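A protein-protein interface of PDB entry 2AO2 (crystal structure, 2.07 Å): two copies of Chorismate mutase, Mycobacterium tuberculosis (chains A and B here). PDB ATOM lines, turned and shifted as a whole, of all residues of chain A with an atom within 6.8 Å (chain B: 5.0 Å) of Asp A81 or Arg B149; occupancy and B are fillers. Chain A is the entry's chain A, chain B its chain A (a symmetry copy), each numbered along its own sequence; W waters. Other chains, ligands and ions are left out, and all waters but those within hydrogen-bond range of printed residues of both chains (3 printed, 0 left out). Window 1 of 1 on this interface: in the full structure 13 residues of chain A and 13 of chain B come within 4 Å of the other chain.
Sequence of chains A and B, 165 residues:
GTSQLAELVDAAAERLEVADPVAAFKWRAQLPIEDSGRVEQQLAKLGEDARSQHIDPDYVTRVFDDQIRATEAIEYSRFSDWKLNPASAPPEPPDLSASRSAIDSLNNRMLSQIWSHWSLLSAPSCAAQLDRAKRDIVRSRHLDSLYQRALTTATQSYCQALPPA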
ATOM      1  N   TRP A  27     -17.932  40.943 -21.132  1.00  0.00           N
ATOM      2  CA  TRP A  27     -17.706  39.772 -22.006  1.00  0.00           C
ATOM      3  C   TRP A  27     -16.781  40.171 -23.156  1.00  0.00           C
ATOM      4  O   TRP A  27     -15.734  39.554 -23.368  1.00  0.00           O
ATOM      5  CB  TRP A  27     -19.034  39.233 -22.510  1.00  0.00           C
ATOM      6  CG  TRP A  27     -18.934  38.058 -23.433  1.00  0.00           C
ATOM      7  CD1 TRP A  27     -18.857  38.095 -24.813  1.00  0.00           C
ATOM      8  CD2 TRP A  27     -18.878  36.666 -23.074  1.00  0.00           C
ATOM      9  NE1 TRP A  27     -18.768  36.813 -25.322  1.00  0.00           N
ATOM     10  CE2 TRP A  27     -18.811  35.917 -24.294  1.00  0.00           C
ATOM     11  CE3 TRP A  27     -18.931  35.979 -21.862  1.00  0.00           C
ATOM     12  CZ2 TRP A  27     -18.721  34.518 -24.321  1.00  0.00           C
ATOM     13  CZ3 TRP A  27     -18.887  34.606 -21.888  1.00  0.00           C
ATOM     14  CH2 TRP A  27     -18.770  33.889 -23.116  1.00  0.00           C
ATOM     15  N   TYR A  76     -23.321  36.679 -13.990  1.00  0.00           N
ATOM     16  CA  TYR A  76     -22.937  35.283 -14.065  1.00  0.00           C
ATOM     17  C   TYR A  76     -23.841  34.414 -14.918  1.00  0.00           C
ATOM     18  O   TYR A  76     -23.381  33.534 -15.610  1.00  0.00           O
ATOM     19  CB  TYR A  76     -22.876  34.670 -12.682  1.00  0.00           C
ATOM     20  CG  TYR A  76     -21.580  34.967 -11.959  1.00  0.00           C
ATOM     21  CD1 TYR A  76     -20.357  34.649 -12.544  1.00  0.00           C
ATOM     22  CD2 TYR A  76     -21.573  35.491 -10.673  1.00  0.00           C
ATOM     23  CE1 TYR A  76     -19.139  34.876 -11.859  1.00  0.00           C
ATOM     24  CE2 TYR A  76     -20.335  35.719  -9.956  1.00  0.00           C
ATOM     25  CZ  TYR A  76     -19.151  35.440 -10.575  1.00  0.00           C
ATOM     26  OH  TYR A  76     -17.964  35.671  -9.930  1.00  0.00           O
ATOM     27  N   SER A  77     -25.144  34.634 -14.790  1.00  0.00           N
ATOM     28  CA  SER A  77     -26.139  33.925 -15.577  1.00  0.00           C
ATOM     29  C   SER A  77     -25.944  34.245 -17.069  1.00  0.00           C
ATOM     30  O   SER A  77     -26.073  33.338 -17.898  1.00  0.00           O
ATOM     31  CB  SER A  77     -27.528  34.372 -15.139  1.00  0.00           C
ATOM     32  OG  SER A  77     -28.477  33.538 -15.766  1.00  0.00           O
ATOM     33  N   ARG A  78     -25.635  35.518 -17.393  1.00  0.00           N
ATOM     34  CA  ARG A  78     -25.387  35.884 -18.777  1.00  0.00           C
ATOM     35  C   ARG A  78     -24.137  35.209 -19.331  1.00  0.00           C
ATOM     36  O   ARG A  78     -24.126  34.759 -20.485  1.00  0.00           O
ATOM     37  CB  ARG A  78     -25.223  37.390 -18.958  1.00  0.00           C
ATOM     38  CG  ARG A  78     -26.435  38.243 -18.666  1.00  0.00           C
ATOM     39  CD  ARG A  78     -27.744  37.551 -19.027  1.00  0.00           C
ATOM     40  NE  ARG A  78     -28.859  38.492 -18.972  1.00  0.00           N
ATOM     41  CZ  ARG A  78     -30.152  38.166 -18.978  1.00  0.00           C
ATOM     42  NH1 ARG A  78     -30.553  36.905 -18.967  1.00  0.00           N
ATOM     43  NH2 ARG A  78     -31.057  39.112 -18.967  1.00  0.00           N
ATOM     44  N   PHE A  79     -23.080  35.175 -18.514  1.00  0.00           N
ATOM     45  CA  PHE A  79     -21.853  34.506 -18.885  1.00  0.00           C
ATOM     46  C   PHE A  79     -22.048  32.991 -19.146  1.00  0.00           C
ATOM     47  O   PHE A  79     -21.487  32.450 -20.105  1.00  0.00           O
ATOM     48  CB  PHE A  79     -20.756  34.734 -17.856  1.00  0.00           C
ATOM     49  CG  PHE A  79     -19.924  35.955 -18.136  1.00  0.00           C
ATOM     50  CD1 PHE A  79     -20.534  37.179 -18.464  1.00  0.00           C
ATOM     51  CD2 PHE A  79     -18.538  35.921 -18.019  1.00  0.00           C
ATOM     52  CE1 PHE A  79     -19.791  38.336 -18.691  1.00  0.00           C
ATOM     53  CE2 PHE A  79     -17.780  37.078 -18.264  1.00  0.00           C
ATOM     54  CZ  PHE A  79     -18.430  38.300 -18.566  1.00  0.00           C
ATOM     55  N   SER A  80     -22.872  32.353 -18.327  1.00  0.00           N
ATOM     56  CA  SER A  80     -23.298  30.988 -18.531  1.00  0.00           C
ATOM     57  C   SER A  80     -23.982  30.826 -19.886  1.00  0.00           C
ATOM     58  O   SER A  80     -23.595  29.976 -20.651  1.00  0.00           O
ATOM     59  CB  SER A  80     -24.251  30.571 -17.433  1.00  0.00           C
ATOM     60  OG  SER A  80     -24.608  29.223 -17.595  1.00  0.00           O
ATOM     61  N   ASP A  81     -24.934  31.708 -20.186  1.00  0.00           N
ATOM     62  CA  ASP A  81     -25.631  31.678 -21.465  1.00  0.00           C
ATOM     63  C   ASP A  81     -24.686  31.825 -22.669  1.00  0.00           C
ATOM     64  O   ASP A  81     -24.833  31.132 -23.694  1.00  0.00           O
ATOM     65  CB  ASP A  81     -26.708  32.757 -21.483  1.00  0.00           C
ATOM     66  CG  ASP A  81     -27.889  32.450 -20.545  1.00  0.00           C
ATOM     67  OD1 ASP A  81     -28.124  31.278 -20.115  1.00  0.00           O
ATOM     68  OD2 ASP A  81     -28.654  33.403 -20.305  1.00  0.00           O
ATOM     69  N   TRP A  82     -23.754  32.766 -22.573  1.00  0.00           N
ATOM     70  CA  TRP A  82     -22.871  33.080 -23.671  1.00  0.00           C
ATOM     71  C   TRP A  82     -21.758  32.079 -23.833  1.00  0.00           C
ATOM     72  O   TRP A  82     -21.199  31.958 -24.903  1.00  0.00           O
ATOM     73  CB  TRP A  82     -22.329  34.499 -23.544  1.00  0.00           C
ATOM     74  CG  TRP A  82     -23.461  35.532 -23.493  1.00  0.00           C
ATOM     75  CD1 TRP A  82     -24.688  35.410 -24.076  1.00  0.00           C
ATOM     76  CD2 TRP A  82     -23.453  36.837 -22.847  1.00  0.00           C
ATOM     77  NE1 TRP A  82     -25.445  36.519 -23.810  1.00  0.00           N
ATOM     78  CE2 TRP A  82     -24.718  37.414 -23.072  1.00  0.00           C
ATOM     79  CE3 TRP A  82     -22.531  37.527 -22.052  1.00  0.00           C
ATOM     80  CZ2 TRP A  82     -25.086  38.662 -22.541  1.00  0.00           C
ATOM     81  CZ3 TRP A  82     -22.879  38.795 -21.570  1.00  0.00           C
ATOM     82  CH2 TRP A  82     -24.147  39.345 -21.810  1.00  0.00           C
ATOM     83  N   LYS A  83     -21.423  31.362 -22.776  1.00  0.00           N
ATOM     84  CA  LYS A  83     -20.541  30.222 -22.917  1.00  0.00           C
ATOM     85  C   LYS A  83     -21.214  29.133 -23.753  1.00  0.00           C
ATOM     86  O   LYS A  83     -20.573  28.552 -24.615  1.00  0.00           O
ATOM     87  CB  LYS A  83     -20.124  29.679 -21.569  1.00  0.00           C
ATOM     88  CG  LYS A  83     -19.088  30.541 -20.918  1.00  0.00           C
ATOM     89  CD  LYS A  83     -17.739  30.309 -21.559  1.00  0.00           C
ATOM     90  CE  LYS A  83     -16.647  31.192 -20.962  1.00  0.00           C
ATOM     91  NZ  LYS A  83     -15.292  30.789 -21.524  1.00  0.00           N
ATOM     92  N   LEU A  84     -22.497  28.878 -23.490  1.00  0.00           N
ATOM     93  CA  LEU A  84     -23.223  27.871 -24.257  1.00  0.00           C
ATOM     94  C   LEU A  84     -23.466  28.366 -25.671  1.00  0.00           C
ATOM     95  O   LEU A  84     -23.415  27.597 -26.620  1.00  0.00           O
ATOM     96  CB  LEU A  84     -24.530  27.485 -23.538  1.00  0.00           C
ATOM     97  CG  LEU A  84     -24.275  26.893 -22.146  1.00  0.00           C
ATOM     98  CD1 LEU A  84     -25.536  26.691 -21.374  1.00  0.00           C
ATOM     99  CD2 LEU A  84     -23.519  25.552 -22.212  1.00  0.00           C
ATOM    100  N   ASN A  85     -23.721  29.659 -25.816  1.00  0.00           N
ATOM    101  CA  ASN A  85     -24.132  30.231 -27.069  1.00  0.00           C
ATOM    102  C   ASN A  85     -23.513  31.585 -27.295  1.00  0.00           C
ATOM    103  O   ASN A  85     -24.207  32.622 -27.186  1.00  0.00           O
ATOM    104  CB  ASN A  85     -25.659  30.397 -27.159  1.00  0.00           C
ATOM    105  CG  ASN A  85     -26.127  30.813 -28.588  1.00  0.00           C
ATOM    106  OD1 ASN A  85     -25.358  30.709 -29.550  1.00  0.00           O
ATOM    107  ND2 ASN A  85     -27.374  31.308 -28.700  1.00  0.00           N
ATOM    108  N   PRO A  86     -22.227  31.579 -27.647  1.00  0.00           N
ATOM    109  CA  PRO A  86     -21.485  32.790 -27.879  1.00  0.00           C
ATOM    110  C   PRO A  86     -22.053  33.734 -28.971  1.00  0.00           C
ATOM    111  O   PRO A  86     -21.878  34.930 -28.839  1.00  0.00           O
ATOM    112  CB  PRO A  86     -20.056  32.282 -28.175  1.00  0.00           C
ATOM    113  CG  PRO A  86     -20.207  30.832 -28.531  1.00  0.00           C
ATOM    114  CD  PRO A  86     -21.399  30.362 -27.817  1.00  0.00           C
ATOM    115  N   SER A  88     -25.064  34.691 -29.204  1.00  0.00           N
ATOM    116  CA  SER A  88     -26.056  35.540 -28.599  1.00  0.00           C
ATOM    117  C   SER A  88     -25.483  36.702 -27.716  1.00  0.00           C
ATOM    118  O   SER A  88     -26.240  37.538 -27.231  1.00  0.00           O
ATOM    119  CB  SER A  88     -27.013  34.663 -27.759  1.00  0.00           C
ATOM    120  OG  SER A  88     -26.402  34.143 -26.596  1.00  0.00           O
ATOM    121  N   ALA A  89     -24.169  36.726 -27.463  1.00  0.00           N
ATOM    122  CA  ALA A  89     -23.569  37.846 -26.719  1.00  0.00           C
ATOM    123  C   ALA A  89     -23.763  39.151 -27.514  1.00  0.00           C
ATOM    124  O   ALA A  89     -23.455  39.201 -28.709  1.00  0.00           O
ATOM    125  CB  ALA A  89     -22.157  37.590 -26.487  1.00  0.00           C
ATOM    126  N   LEU A 146     -35.363  35.364 -13.614  1.00  0.00           N
ATOM    127  CA  LEU A 146     -34.049  35.714 -13.109  1.00  0.00           C
ATOM    128  C   LEU A 146     -34.033  37.083 -12.366  1.00  0.00           C
ATOM    129  O   LEU A 146     -33.514  37.232 -11.251  1.00  0.00           O
ATOM    130  CB  LEU A 146     -33.061  35.805 -14.279  1.00  0.00           C
ATOM    131  CG  LEU A 146     -31.611  36.266 -13.948  1.00  0.00           C
ATOM    132  CD1 LEU A 146     -30.929  35.392 -12.894  1.00  0.00           C
ATOM    133  CD2 LEU A 146     -30.687  36.376 -15.173  1.00  0.00           C
ATOM    134  N   SER B 145     -32.454  20.700 -17.627  1.00  0.00           N
ATOM    135  CA  SER B 145     -32.364  21.610 -18.763  1.00  0.00           C
ATOM    136  C   SER B 145     -30.960  22.227 -18.997  1.00  0.00           C
ATOM    137  O   SER B 145     -30.523  22.345 -20.145  1.00  0.00           O
ATOM    138  CB  SER B 145     -33.382  22.735 -18.588  1.00  0.00           C
ATOM    139  OG  SER B 145     -32.984  23.823 -19.396  1.00  0.00           O
ATOM    140  N   LEU B 146     -30.285  22.639 -17.916  1.00  0.00           N
ATOM    141  CA  LEU B 146     -28.949  23.200 -17.987  1.00  0.00           C
ATOM    142  C   LEU B 146     -27.903  22.196 -18.556  1.00  0.00           C
ATOM    143  O   LEU B 146     -27.106  22.499 -19.455  1.00  0.00           O
ATOM    144  CB  LEU B 146     -28.492  23.606 -16.580  1.00  0.00           C
ATOM    145  CG  LEU B 146     -27.037  24.142 -16.435  1.00  0.00           C
ATOM    146  CD1 LEU B 146     -26.751  25.350 -17.330  1.00  0.00           C
ATOM    147  CD2 LEU B 146     -26.632  24.489 -14.992  1.00  0.00           C
ATOM    148  N   TYR B 147     -27.868  21.025 -17.935  1.00  0.00           N
ATOM    149  CA  TYR B 147     -26.984  19.955 -18.391  1.00  0.00           C
ATOM    150  C   TYR B 147     -27.269  19.508 -19.833  1.00  0.00           C
ATOM    151  O   TYR B 147     -26.333  19.082 -20.550  1.00  0.00           O
ATOM    152  CB  TYR B 147     -27.043  18.787 -17.436  1.00  0.00           C
ATOM    153  CG  TYR B 147     -26.043  18.975 -16.321  1.00  0.00           C
ATOM    154  CD1 TYR B 147     -26.352  19.736 -15.174  1.00  0.00           C
ATOM    155  CD2 TYR B 147     -24.785  18.466 -16.431  1.00  0.00           C
ATOM    156  CE1 TYR B 147     -25.430  19.884 -14.150  1.00  0.00           C
ATOM    157  CE2 TYR B 147     -23.844  18.650 -15.452  1.00  0.00           C
ATOM    158  CZ  TYR B 147     -24.159  19.342 -14.300  1.00  0.00           C
ATOM    159  OH  TYR B 147     -23.150  19.482 -13.327  1.00  0.00           O
ATOM    160  N   GLN B 148     -28.544  19.548 -20.223  1.00  0.00           N
ATOM    161  CA  GLN B 148     -28.937  19.300 -21.620  1.00  0.00           C
ATOM    162  C   GLN B 148     -28.295  20.310 -22.603  1.00  0.00           C
ATOM    163  O   GLN B 148     -27.753  19.931 -23.627  1.00  0.00           O
ATOM    164  CB  GLN B 148     -30.452  19.287 -21.757  1.00  0.00           C
ATOM    165  CG  GLN B 148     -31.057  17.991 -21.232  1.00  0.00           C
ATOM    166  CD  GLN B 148     -32.577  18.000 -21.204  1.00  0.00           C
ATOM    167  OE1 GLN B 148     -33.226  18.285 -22.212  1.00  0.00           O
ATOM    168  NE2 GLN B 148     -33.153  17.665 -20.044  1.00  0.00           N
ATOM    169  N   ARG B 149     -28.316  21.589 -22.245  1.00  0.00           N
ATOM    170  CA  ARG B 149     -27.740  22.628 -23.072  1.00  0.00           C
ATOM    171  C   ARG B 149     -26.256  22.486 -23.144  1.00  0.00           C
ATOM    172  O   ARG B 149     -25.643  22.582 -24.220  1.00  0.00           O
ATOM    173  CB  ARG B 149     -28.113  23.985 -22.537  1.00  0.00           C
ATOM    174  CG  ARG B 149     -29.567  24.329 -22.785  1.00  0.00           C
ATOM    175  CD  ARG B 149     -30.035  25.346 -21.775  1.00  0.00           C
ATOM    176  NE  ARG B 149     -29.413  26.635 -22.035  1.00  0.00           N
ATOM    177  CZ  ARG B 149     -29.090  27.544 -21.120  1.00  0.00           C
ATOM    178  NH1 ARG B 149     -29.322  27.341 -19.817  1.00  0.00           N
ATOM    179  NH2 ARG B 149     -28.510  28.673 -21.522  1.00  0.00           N
ATOM    180  N   ALA B 150     -25.674  22.219 -21.986  1.00  0.00           N
ATOM    181  CA  ALA B 150     -24.257  21.916 -21.906  1.00  0.00           C
ATOM    182  C   ALA B 150     -23.788  20.718 -22.701  1.00  0.00           C
ATOM    183  O   ALA B 150     -22.731  20.756 -23.356  1.00  0.00           O
ATOM    184  CB  ALA B 150     -23.850  21.761 -20.456  1.00  0.00           C
ATOM    185  N   LEU B 151     -24.516  19.632 -22.612  1.00  0.00           N
ATOM    186  CA  LEU B 151     -24.164  18.438 -23.384  1.00  0.00           C
ATOM    187  C   LEU B 151     -24.224  18.709 -24.893  1.00  0.00           C
ATOM    188  O   LEU B 151     -23.441  18.161 -25.649  1.00  0.00           O
ATOM    189  CB  LEU B 151     -25.091  17.284 -23.097  1.00  0.00           C
ATOM    190  CG  LEU B 151     -24.624  15.939 -23.713  1.00  0.00           C
ATOM    191  CD1 LEU B 151     -23.286  15.527 -23.077  1.00  0.00           C
ATOM    192  CD2 LEU B 151     -25.648  14.887 -23.443  1.00  0.00           C
ATOM    193  N   THR B 152     -25.190  19.504 -25.317  1.00  0.00           N
ATOM    194  CA  THR B 152     -25.267  19.962 -26.737  1.00  0.00           C
ATOM    195  C   THR B 152     -24.009  20.789 -27.117  1.00  0.00           C
ATOM    196  O   THR B 152     -23.392  20.553 -28.120  1.00  0.00           O
ATOM    197  CB  THR B 152     -26.571  20.748 -26.970  1.00  0.00           C
ATOM    198  OG1 THR B 152     -27.660  19.834 -26.898  1.00  0.00           O
ATOM    199  CG2 THR B 152     -26.612  21.439 -28.394  1.00  0.00           C
ATOM    200  N   THR B 153     -23.591  21.720 -26.270  1.00  0.00           N
ATOM    201  CA  THR B 153     -22.390  22.507 -26.538  1.00  0.00           C
ATOM    202  C   THR B 153     -21.152  21.595 -26.605  1.00  0.00           C
ATOM    203  O   THR B 153     -20.331  21.720 -27.505  1.00  0.00           O
ATOM    204  CB  THR B 153     -22.217  23.620 -25.435  1.00  0.00           C
ATOM    205  OG1 THR B 153     -23.356  24.478 -25.445  1.00  0.00           O
ATOM    206  CG2 THR B 153     -21.021  24.450 -25.649  1.00  0.00           C
HETATM  207  O   HOH W   1     -27.229  29.763 -24.059  1.00  0.00           O
HETATM  208  O   HOH W   2     -24.663  25.134 -27.952  1.00  0.00           O
HETATM  209  O   HOH W   3     -27.244  29.304 -18.483  1.00  0.00           O
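The side-chain carboxylate of Asp A81 is in salt-bridge range of the guanidinium group of Arg B149 (3.0 Å).
The backbone carbonyl oxygen (O) of Leu A84 sits at hydrogen-bond distance from the side-chain hydroxyl (OG1) of Thr B153, 3.3 Å away.
O of Arg B149 lies within hydrogen-bond range of OG1 of Thr B153 (3.2 Å).
Among the printed residues, pairs that only touch across the chains: Leu A84 with Arg B149 and Leu A84 with Ala B150.
Of the printed residues of chain B, Asp A81 touches Arg B149.
Of the printed residues of chain B, Leu A84 touches Arg B149 (3.6 Å), Ala B150 (3.7 Å) and Thr B153 (3.3 Å).
Arg B149 touches two residues of chain A.
Of the printed residues of chain A, Ala B150 touches Leu A84.
Of the printed residues of chain A, Thr B153 touches Leu A84 (3.3 Å).
Hydrophobic or aromatic side chains of chain A that line the printed part of chain B: Leu A84.
Among the printed residues, Asp or Glu carboxylates within 4 Å of a Lys or Arg side-chain nitrogen of the other chain: Asp A81 with Arg B149 (3.0 Å).
Position printed for both chains: 146.
Water W3 lies within hydrogen-bond range of OD1 of Asp A81, OG of Ser A80 and NH1 of Arg B149.
Water W1 lies within hydrogen-bond range of the backbone carbonyl oxygen of Asp A81 (2.8 Å) and the guanidinium group of Arg B149 (3.0 Å).
Water W2 lies within hydrogen-bond range of OG1 of Thr B153 and O of Leu A84.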
